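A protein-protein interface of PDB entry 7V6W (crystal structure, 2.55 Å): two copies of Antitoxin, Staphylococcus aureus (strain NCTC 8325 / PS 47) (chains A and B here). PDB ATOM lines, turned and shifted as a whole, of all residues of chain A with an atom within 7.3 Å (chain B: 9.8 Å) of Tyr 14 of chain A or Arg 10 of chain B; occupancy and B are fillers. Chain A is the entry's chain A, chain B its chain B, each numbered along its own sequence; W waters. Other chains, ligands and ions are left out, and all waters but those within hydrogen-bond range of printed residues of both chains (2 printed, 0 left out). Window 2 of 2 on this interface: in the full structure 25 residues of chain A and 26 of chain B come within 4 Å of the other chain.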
ATOM      1  N   ALA A   9       5.493   5.260  -0.934  1.00  0.00           N
ATOM      2  CA  ALA A   9       5.854   5.243   0.479  1.00  0.00           C
ATOM      3  C   ALA A   9       4.644   4.997   1.367  1.00  0.00           C
ATOM      4  O   ALA A   9       4.772   4.373   2.425  1.00  0.00           O
ATOM      5  CB  ALA A   9       6.528   6.558   0.869  1.00  0.00           C
ATOM      6  N   ARG A  10       3.469   5.483   0.968  1.00  0.00           N
ATOM      7  CA  ARG A  10       2.293   5.321   1.814  1.00  0.00           C
ATOM      8  C   ARG A  10       1.750   3.899   1.757  1.00  0.00           C
ATOM      9  O   ARG A  10       1.092   3.454   2.703  1.00  0.00           O
ATOM     10  CB  ARG A  10       1.215   6.326   1.413  1.00  0.00           C
ATOM     11  CG  ARG A  10       0.167   6.573   2.485  1.00  0.00           C
ATOM     12  CD  ARG A  10      -0.989   7.406   1.956  1.00  0.00           C
ATOM     13  NE  ARG A  10      -1.779   6.674   0.971  1.00  0.00           N
ATOM     14  CZ  ARG A  10      -2.910   7.122   0.434  1.00  0.00           C
ATOM     15  NH1 ARG A  10      -3.392   8.306   0.786  1.00  0.00           N
ATOM     16  NH2 ARG A  10      -3.562   6.383  -0.454  1.00  0.00           N
ATOM     17  N   LYS A  11       2.022   3.175   0.670  1.00  0.00           N
ATOM     18  CA  LYS A  11       1.590   1.786   0.569  1.00  0.00           C
ATOM     19  C   LYS A  11       2.363   0.886   1.522  1.00  0.00           C
ATOM     20  O   LYS A  11       1.808  -0.095   2.032  1.00  0.00           O
ATOM     21  CB  LYS A  11       1.743   1.288  -0.869  1.00  0.00           C
ATOM     22  CG  LYS A  11       0.760   1.904  -1.848  1.00  0.00           C
ATOM     23  CD  LYS A  11       0.991   1.377  -3.252  1.00  0.00           C
ATOM     24  CE  LYS A  11       0.087   2.057  -4.263  1.00  0.00           C
ATOM     25  NZ  LYS A  11       0.327   1.540  -5.639  1.00  0.00           N
ATOM     26  N   ASP A  12       3.632   1.191   1.769  1.00  0.00           N
ATOM     27  CA  ASP A  12       4.462   0.444   2.708  1.00  0.00           C
ATOM     28  C   ASP A  12       5.053   1.392   3.744  1.00  0.00           C
ATOM     29  O   ASP A  12       6.263   1.431   3.982  1.00  0.00           O
ATOM     30  CB  ASP A  12       5.555  -0.325   1.972  1.00  0.00           C
ATOM     31  CG  ASP A  12       5.749  -1.724   2.522  1.00  0.00           C
ATOM     32  OD1 ASP A  12       5.023  -2.099   3.467  1.00  0.00           O
ATOM     33  OD2 ASP A  12       6.626  -2.448   2.007  1.00  0.00           O
ATOM     34  N   PHE A  13       4.177   2.173   4.378  1.00  0.00           N
ATOM     35  CA  PHE A  13       4.624   3.196   5.318  1.00  0.00           C
ATOM     36  C   PHE A  13       5.232   2.578   6.570  1.00  0.00           C
ATOM     37  O   PHE A  13       6.281   3.030   7.046  1.00  0.00           O
ATOM     38  CB  PHE A  13       3.451   4.110   5.674  1.00  0.00           C
ATOM     39  CG  PHE A  13       3.846   5.330   6.453  1.00  0.00           C
ATOM     40  CD1 PHE A  13       4.645   6.305   5.878  1.00  0.00           C
ATOM     41  CD2 PHE A  13       3.407   5.509   7.754  1.00  0.00           C
ATOM     42  CE1 PHE A  13       5.009   7.429   6.591  1.00  0.00           C
ATOM     43  CE2 PHE A  13       3.765   6.633   8.471  1.00  0.00           C
ATOM     44  CZ  PHE A  13       4.568   7.596   7.889  1.00  0.00           C
ATOM     45  N   TYR A  14       4.594   1.540   7.115  1.00  0.00           N
ATOM     46  CA  TYR A  14       5.098   0.926   8.339  1.00  0.00           C
ATOM     47  C   TYR A  14       6.424   0.214   8.100  1.00  0.00           C
ATOM     48  O   TYR A  14       7.335   0.292   8.933  1.00  0.00           O
ATOM     49  CB  TYR A  14       4.057  -0.038   8.907  1.00  0.00           C
ATOM     50  CG  TYR A  14       2.753   0.634   9.273  1.00  0.00           C
ATOM     51  CD1 TYR A  14       2.607   1.292  10.488  1.00  0.00           C
ATOM     52  CD2 TYR A  14       1.669   0.615   8.403  1.00  0.00           C
ATOM     53  CE1 TYR A  14       1.420   1.910  10.829  1.00  0.00           C
ATOM     54  CE2 TYR A  14       0.475   1.233   8.737  1.00  0.00           C
ATOM     55  CZ  TYR A  14       0.358   1.877   9.952  1.00  0.00           C
ATOM     56  OH  TYR A  14      -0.824   2.493  10.297  1.00  0.00           O
ATOM     57  N   GLN A  15       6.556  -0.487   6.971  1.00  0.00           N
ATOM     58  CA  GLN A  15       7.829  -1.128   6.662  1.00  0.00           C
ATOM     59  C   GLN A  15       8.921  -0.098   6.408  1.00  0.00           C
ATOM     60  O   GLN A  15      10.094  -0.352   6.709  1.00  0.00           O
ATOM     61  CB  GLN A  15       7.675  -2.054   5.456  1.00  0.00           C
ATOM     62  CG  GLN A  15       8.878  -2.946   5.212  1.00  0.00           C
ATOM     63  CD  GLN A  15       9.172  -3.852   6.391  1.00  0.00           C
ATOM     64  OE1 GLN A  15       8.275  -4.500   6.930  1.00  0.00           O
ATOM     65  NE2 GLN A  15      10.434  -3.895   6.804  1.00  0.00           N
ATOM     66  N   LEU A  16       8.556   1.064   5.864  1.00  0.00           N
ATOM     67  CA  LEU A  16       9.528   2.133   5.661  1.00  0.00           C
ATOM     68  C   LEU A  16      10.109   2.598   6.991  1.00  0.00           C
ATOM     69  O   LEU A  16      11.330   2.746   7.132  1.00  0.00           O
ATOM     70  CB  LEU A  16       8.864   3.294   4.915  1.00  0.00           C
ATOM     71  CG  LEU A  16       9.711   4.437   4.350  1.00  0.00           C
ATOM     72  CD1 LEU A  16       8.948   5.142   3.245  1.00  0.00           C
ATOM     73  CD2 LEU A  16      10.105   5.440   5.426  1.00  0.00           C
ATOM     74  N   LEU A  17       9.243   2.837   7.980  1.00  0.00           N
ATOM     75  CA  LEU A  17       9.705   3.310   9.281  1.00  0.00           C
ATOM     76  C   LEU A  17      10.590   2.281   9.975  1.00  0.00           C
ATOM     77  O   LEU A  17      11.536   2.654  10.677  1.00  0.00           O
ATOM     78  CB  LEU A  17       8.507   3.663  10.163  1.00  0.00           C
ATOM     79  CG  LEU A  17       7.588   4.750   9.602  1.00  0.00           C
ATOM     80  CD1 LEU A  17       6.389   4.954  10.509  1.00  0.00           C
ATOM     81  CD2 LEU A  17       8.355   6.049   9.419  1.00  0.00           C
ATOM     82  N   LYS A  18      10.302   0.990   9.797  1.00  0.00           N
ATOM     83  CA  LYS A  18      11.172  -0.034  10.365  1.00  0.00           C
ATOM     84  C   LYS A  18      12.515  -0.073   9.644  1.00  0.00           C
ATOM     85  O   LYS A  18      13.565  -0.222  10.281  1.00  0.00           O
ATOM     86  CB  LYS A  18      10.488  -1.401  10.306  1.00  0.00           C
ATOM     87  CG  LYS A  18       9.140  -1.449  11.010  1.00  0.00           C
ATOM     88  CD  LYS A  18       8.421  -2.773  10.784  1.00  0.00           C
ATOM     89  CE  LYS A  18       7.065  -2.778  11.480  1.00  0.00           C
ATOM     90  NZ  LYS A  18       6.320  -4.048  11.264  1.00  0.00           N
ATOM     91  N   ASN A  19      12.500   0.074   8.316  1.00  0.00           N
ATOM     92  CA  ASN A  19      13.731  -0.025   7.538  1.00  0.00           C
ATOM     93  C   ASN A  19      14.685   1.122   7.846  1.00  0.00           C
ATOM     94  O   ASN A  19      15.904   0.922   7.892  1.00  0.00           O
ATOM     95  CB  ASN A  19      13.407  -0.061   6.045  1.00  0.00           C
ATOM     96  CG  ASN A  19      12.861  -1.400   5.600  1.00  0.00           C
ATOM     97  OD1 ASN A  19      12.493  -2.237   6.423  1.00  0.00           O
ATOM     98  ND2 ASN A  19      12.805  -1.612   4.291  1.00  0.00           N
ATOM     99  N   VAL A  20      14.155   2.329   8.057  1.00  0.00           N
ATOM    100  CA  VAL A  20      15.022   3.470   8.326  1.00  0.00           C
ATOM    101  C   VAL A  20      15.715   3.339   9.677  1.00  0.00           C
ATOM    102  O   VAL A  20      16.764   3.956   9.894  1.00  0.00           O
ATOM    103  CB  VAL A  20      14.225   4.787   8.234  1.00  0.00           C
ATOM    104  CG1 VAL A  20      13.417   5.028   9.503  1.00  0.00           C
ATOM    105  CG2 VAL A  20      15.154   5.952   7.959  1.00  0.00           C
ATOM    106  N   THR B   4       3.270  12.821  16.104  1.00  0.00           N
ATOM    107  CA  THR B   4       2.133  12.059  15.610  1.00  0.00           C
ATOM    108  C   THR B   4       2.489  10.580  15.573  1.00  0.00           C
ATOM    109  O   THR B   4       3.663  10.202  15.529  1.00  0.00           O
ATOM    110  CB  THR B   4       1.694  12.535  14.219  1.00  0.00           C
ATOM    111  OG1 THR B   4       0.615  11.719  13.749  1.00  0.00           O
ATOM    112  CG2 THR B   4       2.852  12.448  13.236  1.00  0.00           C
ATOM    113  N   SER B   5       1.457   9.746  15.595  1.00  0.00           N
ATOM    114  CA  SER B   5       1.630   8.309  15.492  1.00  0.00           C
ATOM    115  C   SER B   5       1.835   7.906  14.035  1.00  0.00           C
ATOM    116  O   SER B   5       1.463   8.646  13.120  1.00  0.00           O
ATOM    117  CB  SER B   5       0.412   7.594  16.064  1.00  0.00           C
ATOM    118  OG  SER B   5      -0.731   7.834  15.262  1.00  0.00           O
ATOM    119  N   PRO B   6       2.437   6.737  13.790  1.00  0.00           N
ATOM    120  CA  PRO B   6       2.582   6.283  12.395  1.00  0.00           C
ATOM    121  C   PRO B   6       1.254   6.165  11.668  1.00  0.00           C
ATOM    122  O   PRO B   6       1.154   6.565  10.501  1.00  0.00           O
ATOM    123  CB  PRO B   6       3.276   4.920  12.542  1.00  0.00           C
ATOM    124  CG  PRO B   6       3.967   4.982  13.861  1.00  0.00           C
ATOM    125  CD  PRO B   6       3.093   5.823  14.742  1.00  0.00           C
ATOM    126  N   THR B   7       0.224   5.638  12.337  1.00  0.00           N
ATOM    127  CA  THR B   7      -1.084   5.496  11.704  1.00  0.00           C
ATOM    128  C   THR B   7      -1.688   6.854  11.368  1.00  0.00           C
ATOM    129  O   THR B   7      -2.230   7.044  10.271  1.00  0.00           O
ATOM    130  CB  THR B   7      -2.021   4.695  12.611  1.00  0.00           C
ATOM    131  OG1 THR B   7      -1.475   3.388  12.828  1.00  0.00           O
ATOM    132  CG2 THR B   7      -3.399   4.562  11.978  1.00  0.00           C
ATOM    133  N   GLU B   8      -1.609   7.813  12.294  1.00  0.00           N
ATOM    134  CA  GLU B   8      -2.083   9.160  11.992  1.00  0.00           C
ATOM    135  C   GLU B   8      -1.234   9.812  10.909  1.00  0.00           C
ATOM    136  O   GLU B   8      -1.752  10.552  10.065  1.00  0.00           O
ATOM    137  CB  GLU B   8      -2.090  10.018  13.256  1.00  0.00           C
ATOM    138  CG  GLU B   8      -3.315   9.834  14.134  1.00  0.00           C
ATOM    139  CD  GLU B   8      -4.606  10.141  13.399  1.00  0.00           C
ATOM    140  OE1 GLU B   8      -5.271   9.189  12.938  1.00  0.00           O
ATOM    141  OE2 GLU B   8      -4.950  11.337  13.274  1.00  0.00           O
ATOM    142  N   ALA B   9       0.076   9.548  10.918  1.00  0.00           N
ATOM    143  CA  ALA B   9       0.941  10.090   9.877  1.00  0.00           C
ATOM    144  C   ALA B   9       0.584   9.533   8.507  1.00  0.00           C
ATOM    145  O   ALA B   9       0.708  10.240   7.502  1.00  0.00           O
ATOM    146  CB  ALA B   9       2.407   9.802  10.204  1.00  0.00           C
ATOM    147  N   ARG B  10       0.133   8.276   8.443  1.00  0.00           N
ATOM    148  CA  ARG B  10      -0.244   7.700   7.157  1.00  0.00           C
ATOM    149  C   ARG B  10      -1.530   8.318   6.622  1.00  0.00           C
ATOM    150  O   ARG B  10      -1.692   8.449   5.403  1.00  0.00           O
ATOM    151  CB  ARG B  10      -0.393   6.183   7.280  1.00  0.00           C
ATOM    152  CG  ARG B  10      -0.266   5.444   5.956  1.00  0.00           C
ATOM    153  CD  ARG B  10      -0.529   3.952   6.105  1.00  0.00           C
ATOM    154  NE  ARG B  10      -1.939   3.671   6.355  1.00  0.00           N
ATOM    155  CZ  ARG B  10      -2.483   2.459   6.298  1.00  0.00           C
ATOM    156  NH1 ARG B  10      -1.734   1.407   5.996  1.00  0.00           N
ATOM    157  NH2 ARG B  10      -3.778   2.300   6.539  1.00  0.00           N
ATOM    158  N   LYS B  11      -2.448   8.707   7.510  1.00  0.00           N
ATOM    159  CA  LYS B  11      -3.692   9.326   7.065  1.00  0.00           C
ATOM    160  C   LYS B  11      -3.446  10.709   6.474  1.00  0.00           C
ATOM    161  O   LYS B  11      -4.058  11.078   5.466  1.00  0.00           O
ATOM    162  CB  LYS B  11      -4.682   9.415   8.227  1.00  0.00           C
ATOM    163  CG  LYS B  11      -5.140   8.073   8.772  1.00  0.00           C
ATOM    164  CD  LYS B  11      -6.165   8.259   9.883  1.00  0.00           C
ATOM    165  CE  LYS B  11      -6.704   6.924  10.375  1.00  0.00           C
ATOM    166  NZ  LYS B  11      -7.749   7.100  11.421  1.00  0.00           N
ATOM    167  N   ASP B  12      -2.556  11.487   7.086  1.00  0.00           N
ATOM    168  CA  ASP B  12      -2.262  12.851   6.660  1.00  0.00           C
ATOM    169  C   ASP B  12      -0.854  12.961   6.084  1.00  0.00           C
ATOM    170  O   ASP B  12      -0.141  13.935   6.329  1.00  0.00           O
ATOM    171  CB  ASP B  12      -2.433  13.825   7.823  1.00  0.00           C
ATOM    172  CG  ASP B  12      -3.740  13.627   8.561  1.00  0.00           C
ATOM    173  OD1 ASP B  12      -4.765  13.361   7.898  1.00  0.00           O
ATOM    174  OD2 ASP B  12      -3.741  13.731   9.806  1.00  0.00           O
ATOM    175  N   PHE B  13      -0.444  11.962   5.299  1.00  0.00           N
ATOM    176  CA  PHE B  13       0.940  11.896   4.841  1.00  0.00           C
ATOM    177  C   PHE B  13       1.256  13.018   3.859  1.00  0.00           C
ATOM    178  O   PHE B  13       2.272  13.709   4.001  1.00  0.00           O
ATOM    179  CB  PHE B  13       1.217  10.529   4.213  1.00  0.00           C
ATOM    180  CG  PHE B  13       2.666  10.285   3.903  1.00  0.00           C
ATOM    181  CD1 PHE B  13       3.629  10.410   4.892  1.00  0.00           C
ATOM    182  CD2 PHE B  13       3.064   9.915   2.629  1.00  0.00           C
ATOM    183  CE1 PHE B  13       4.964  10.183   4.612  1.00  0.00           C
ATOM    184  CE2 PHE B  13       4.397   9.683   2.343  1.00  0.00           C
ATOM    185  CZ  PHE B  13       5.348   9.817   3.337  1.00  0.00           C
ATOM    186  N   TYR B  14       0.398  13.217   2.857  1.00  0.00           N
ATOM    187  CA  TYR B  14       0.658  14.258   1.868  1.00  0.00           C
ATOM    188  C   TYR B  14       0.597  15.649   2.483  1.00  0.00           C
ATOM    189  O   TYR B  14       1.262  16.570   1.995  1.00  0.00           O
ATOM    190  CB  TYR B  14      -0.333  14.145   0.711  1.00  0.00           C
ATOM    191  CG  TYR B  14      -0.231  12.844  -0.047  1.00  0.00           C
ATOM    192  CD1 TYR B  14       0.642  12.709  -1.120  1.00  0.00           C
ATOM    193  CD2 TYR B  14      -1.004  11.748   0.311  1.00  0.00           C
ATOM    194  CE1 TYR B  14       0.737  11.520  -1.816  1.00  0.00           C
ATOM    195  CE2 TYR B  14      -0.912  10.555  -0.376  1.00  0.00           C
ATOM    196  CZ  TYR B  14      -0.043  10.448  -1.440  1.00  0.00           C
ATOM    197  OH  TYR B  14       0.047   9.261  -2.128  1.00  0.00           O
ATOM    198  N   GLN B  15      -0.188  15.822   3.546  1.00  0.00           N
ATOM    199  CA  GLN B  15      -0.238  17.116   4.212  1.00  0.00           C
ATOM    200  C   GLN B  15       0.961  17.329   5.127  1.00  0.00           C
ATOM    201  O   GLN B  15       1.373  18.474   5.343  1.00  0.00           O
ATOM    202  CB  GLN B  15      -1.541  17.253   5.002  1.00  0.00           C
ATOM    203  CG  GLN B  15      -1.877  18.685   5.372  1.00  0.00           C
ATOM    204  CD  GLN B  15      -1.943  19.595   4.161  1.00  0.00           C
ATOM    205  OE1 GLN B  15      -1.337  20.667   4.141  1.00  0.00           O
ATOM    206  NE2 GLN B  15      -2.681  19.171   3.141  1.00  0.00           N
ATOM    207  N   LEU B  16       1.532  16.249   5.666  1.00  0.00           N
ATOM    208  CA  LEU B  16       2.738  16.381   6.477  1.00  0.00           C
ATOM    209  C   LEU B  16       3.944  16.743   5.620  1.00  0.00           C
ATOM    210  O   LEU B  16       4.792  17.540   6.038  1.00  0.00           O
ATOM    211  CB  LEU B  16       3.004  15.086   7.247  1.00  0.00           C
ATOM    212  CG  LEU B  16       2.096  14.783   8.440  1.00  0.00           C
ATOM    213  CD1 LEU B  16       2.478  13.453   9.071  1.00  0.00           C
ATOM    214  CD2 LEU B  16       2.155  15.907   9.464  1.00  0.00           C
ATOM    215  N   LEU B  17       4.038  16.167   4.417  1.00  0.00           N
ATOM    216  CA  LEU B  17       5.168  16.457   3.541  1.00  0.00           C
ATOM    217  C   LEU B  17       5.188  17.917   3.113  1.00  0.00           C
ATOM    218  O   LEU B  17       6.261  18.473   2.852  1.00  0.00           O
ATOM    219  CB  LEU B  17       5.131  15.545   2.314  1.00  0.00           C
ATOM    220  CG  LEU B  17       5.306  14.048   2.571  1.00  0.00           C
ATOM    221  CD1 LEU B  17       5.200  13.263   1.271  1.00  0.00           C
ATOM    222  CD2 LEU B  17       6.633  13.774   3.262  1.00  0.00           C
ATOM    223  N   ILE B  27       8.659  16.839  11.671  1.00  0.00           N
ATOM    224  CA  ILE B  27       7.528  16.095  12.213  1.00  0.00           C
ATOM    225  C   ILE B  27       8.073  14.830  12.860  1.00  0.00           C
ATOM    226  O   ILE B  27       8.775  14.045  12.212  1.00  0.00           O
ATOM    227  CB  ILE B  27       6.497  15.753  11.127  1.00  0.00           C
ATOM    228  CG1 ILE B  27       6.059  17.012  10.377  1.00  0.00           C
ATOM    229  CG2 ILE B  27       5.292  15.052  11.738  1.00  0.00           C
ATOM    230  CD1 ILE B  27       5.434  18.067  11.250  1.00  0.00           C
ATOM    231  N   ILE B  29       7.530  11.171  14.504  1.00  0.00           N
ATOM    232  CA  ILE B  29       6.625  10.031  14.431  1.00  0.00           C
ATOM    233  C   ILE B  29       6.938   9.121  15.611  1.00  0.00           C
ATOM    234  O   ILE B  29       7.994   8.478  15.650  1.00  0.00           O
ATOM    235  CB  ILE B  29       6.755   9.283  13.098  1.00  0.00           C
ATOM    236  CG1 ILE B  29       6.347  10.193  11.938  1.00  0.00           C
ATOM    237  CG2 ILE B  29       5.923   8.013  13.110  1.00  0.00           C
ATOM    238  CD1 ILE B  29       6.449   9.534  10.583  1.00  0.00           C
ATOM    239  N   SER B  30       6.014   9.060  16.569  1.00  0.00           N
ATOM    240  CA  SER B  30       6.173   8.253  17.772  1.00  0.00           C
ATOM    241  C   SER B  30       4.952   7.357  17.933  1.00  0.00           C
ATOM    242  O   SER B  30       3.821   7.851  18.000  1.00  0.00           O
ATOM    243  CB  SER B  30       6.357   9.134  19.013  1.00  0.00           C
ATOM    244  OG  SER B  30       6.389   8.349  20.198  1.00  0.00           O
ATOM    245  N   GLY B  31       5.175   6.047  18.012  1.00  0.00           N
ATOM    246  CA  GLY B  31       4.074   5.109  18.152  1.00  0.00           C
ATOM    247  C   GLY B  31       4.281   4.076  19.243  1.00  0.00           C
ATOM    248  O   GLY B  31       5.251   4.153  20.004  1.00  0.00           O
ATOM    249  N   ASN B  32       3.373   3.099  19.335  1.00  0.00           N
ATOM    250  CA  ASN B  32       3.476   2.097  20.395  1.00  0.00           C
ATOM    251  C   ASN B  32       4.764   1.292  20.283  1.00  0.00           C
ATOM    252  O   ASN B  32       5.319   0.863  21.300  1.00  0.00           O
ATOM    253  CB  ASN B  32       2.262   1.165  20.371  1.00  0.00           C
ATOM    254  CG  ASN B  32       0.957   1.914  20.477  1.00  0.00           C
ATOM    255  OD1 ASN B  32       0.907   3.029  20.995  1.00  0.00           O
ATOM    256  ND2 ASN B  32      -0.114   1.304  19.985  1.00  0.00           N
ATOM    257  N   ASN B  33       5.253   1.085  19.065  1.00  0.00           N
ATOM    258  CA  ASN B  33       6.530   0.414  18.834  1.00  0.00           C
ATOM    259  C   ASN B  33       7.580   1.508  18.648  1.00  0.00           C
ATOM    260  O   ASN B  33       7.880   1.929  17.530  1.00  0.00           O
ATOM    261  CB  ASN B  33       6.444  -0.519  17.630  1.00  0.00           C
ATOM    262  CG  ASN B  33       5.239  -1.438  17.691  1.00  0.00           C
ATOM    263  OD1 ASN B  33       4.710  -1.717  18.766  1.00  0.00           O
ATOM    264  ND2 ASN B  33       4.794  -1.910  16.530  1.00  0.00           N
ATOM    265  N   GLU B  35      10.707   1.550  18.783  1.00  0.00           N
ATOM    266  CA  GLU B  35      11.895   1.244  17.995  1.00  0.00           C
ATOM    267  C   GLU B  35      11.734   1.644  16.534  1.00  0.00           C
ATOM    268  O   GLU B  35      12.736   1.759  15.821  1.00  0.00           O
ATOM    269  CB  GLU B  35      12.236  -0.246  18.093  1.00  0.00           C
ATOM    270  CG  GLU B  35      11.234  -1.174  17.420  1.00  0.00           C
ATOM    271  CD  GLU B  35      10.034  -1.482  18.296  1.00  0.00           C
ATOM    272  OE1 GLU B  35       9.172  -2.275  17.863  1.00  0.00           O
ATOM    273  OE2 GLU B  35       9.954  -0.934  19.415  1.00  0.00           O
ATOM    274  N   ASN B  36      10.502   1.862  16.079  1.00  0.00           N
ATOM    275  CA  ASN B  36      10.221   2.288  14.716  1.00  0.00           C
ATOM    276  C   ASN B  36       9.961   3.785  14.612  1.00  0.00           C
ATOM    277  O   ASN B  36       9.487   4.250  13.571  1.00  0.00           O
ATOM    278  CB  ASN B  36       9.026   1.511  14.160  1.00  0.00           C
ATOM    279  CG  ASN B  36       9.201   0.011  14.280  1.00  0.00           C
ATOM    280  OD1 ASN B  36      10.293  -0.517  14.070  1.00  0.00           O
ATOM    281  ND2 ASN B  36       8.123  -0.684  14.628  1.00  0.00           N
ATOM    282  N   ASN B  37      10.250   4.544  15.666  1.00  0.00           N
ATOM    283  CA  ASN B  37      10.046   5.984  15.634  1.00  0.00           C
ATOM    284  C   ASN B  37      10.968   6.636  14.609  1.00  0.00           C
ATOM    285  O   ASN B  37      12.094   6.188  14.378  1.00  0.00           O
ATOM    286  CB  ASN B  37      10.283   6.590  17.018  1.00  0.00           C
ATOM    287  CG  ASN B  37       9.149   6.301  17.982  1.00  0.00           C
ATOM    288  OD1 ASN B  37       8.221   5.561  17.660  1.00  0.00           O
ATOM    289  ND2 ASN B  37       9.221   6.882  19.174  1.00  0.00           N
ATOM    290  N   ALA B  38      10.474   7.707  13.992  1.00  0.00           N
ATOM    291  CA  ALA B  38      11.197   8.380  12.925  1.00  0.00           C
ATOM    292  C   ALA B  38      10.852   9.863  12.951  1.00  0.00           C
ATOM    293  O   ALA B  38      10.023  10.317  13.744  1.00  0.00           O
ATOM    294  CB  ALA B  38      10.874   7.754  11.563  1.00  0.00           C
ATOM    295  N   ILE B  40      10.395  13.348  10.079  1.00  0.00           N
ATOM    296  CA  ILE B  40      10.268  13.817   8.703  1.00  0.00           C
ATOM    297  C   ILE B  40      10.822  15.232   8.629  1.00  0.00           C
ATOM    298  O   ILE B  40      10.400  16.111   9.390  1.00  0.00           O
ATOM    299  CB  ILE B  40       8.806  13.784   8.224  1.00  0.00           C
ATOM    300  CG1 ILE B  40       8.107  12.508   8.700  1.00  0.00           C
ATOM    301  CG2 ILE B  40       8.741  13.904   6.708  1.00  0.00           C
ATOM    302  CD1 ILE B  40       8.716  11.241   8.167  1.00  0.00           C
HETATM  303  O   HOH W   1      -2.301   3.725   3.232  1.00  0.00           O
HETATM  304  O   HOH W   2      -2.805  10.448   3.092  1.00  0.00           O
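OH of Tyr 14 of chain A lies within hydrogen-bond range of OG1 of Thr 7 of chain B (2.8 Å).
The backbone NH (N) of Ile 29 of chain B sits at hydrogen-bond distance from the backbone carbonyl oxygen (O) of Ala 38 of chain B (2.7 Å).
Arg 10 of chain A touches Arg 10 of chain B (CD to O, 3.7 Å).
Arg 10 of chain A touches Tyr 14 of chain B (NH1 to CE2, 3.5 Å).
Pro 6 of chain B touches Phe 13 of chain A (O to CE2, 3.3 Å).
Arg 10 of chain B touches Phe 13 of chain A (CB to CD2, 3.9 Å).
Phe 13 of chain A touches Phe 13 of chain B.
CZ of Phe 13 of chain A touches CD1 of Ile 29 of chain B, at 3.8 Å.
Tyr 14 of chain A touches Pro 6 of chain B (CE1 to CB, 3.9 Å).
Leu 17 of chain A touches Asn 36 of chain B.
Ala 38 of chain B touches Leu 17 of chain A.
Asn 36 of chain B touches Lys 18 of chain A (OD1 to CG, 3.4 Å).
Of chain B, only Pro 6, Ala 9, Arg 10, Phe 13 and Ile 29 come within 4 Å of Phe 13 of chain A.
Of the printed residues of chain B, Tyr 14 of chain A touches Pro 6, Thr 7 and Arg 10.
No residue of chain B comes within 4 Å of Gln 15 of chain A.
Asn 19 of chain A touches none of the printed residues of chain B.
Of the printed residues of chain A, Thr 7 of chain B touches Tyr 14.
Of the printed residues of chain A, Ala 9 of chain B touches Phe 13 (3.9 Å).
Arg 10 of chain B touches three residues of chain A.
Leu 17 of chain B touches none of the printed residues of chain A.
The nearest printed residue of chain A that does not touch Phe 13 of chain B is Ala 9 of chain A (4.1 Å).
Along chain A the printed residues that touch a printed residue of chain B span positions 10 to 18.
Among the printed residues, 14 pairs touch across the chains.
Arg 10 of chain B touches its own counterpart, Arg 10 of chain A.
Arg 10 of chain A touches Tyr 14 of chain B, and with the chains exchanged Tyr 14 of chain A touches Arg 10 of chain B.
Phe 13 of chain A touches Arg 10 of chain B, but with the chains exchanged Arg 10 of chain A does not touch Phe 13 of chain B (4.2 Å).
Phe 13 of chain A touches its own counterpart, Phe 13 of chain B.
9 positions are printed for both chains.
Of the 14 pairs that touch across the chains among the printed residues, 4 have their exchanged pair printed and touching as well.
Water W2 lies within hydrogen-bond range of O of Lys 11 of chain B (2.8 Å), NH1 of Arg 10 of chain A (3.2 Å) and O of Arg 10 of chain B (3.3 Å).
Water W1 bridges the guanidinium group of Arg 10 of chain B (3.1 Å) and the backbone carbonyl oxygen of Arg 10 of chain A (3.4 Å).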
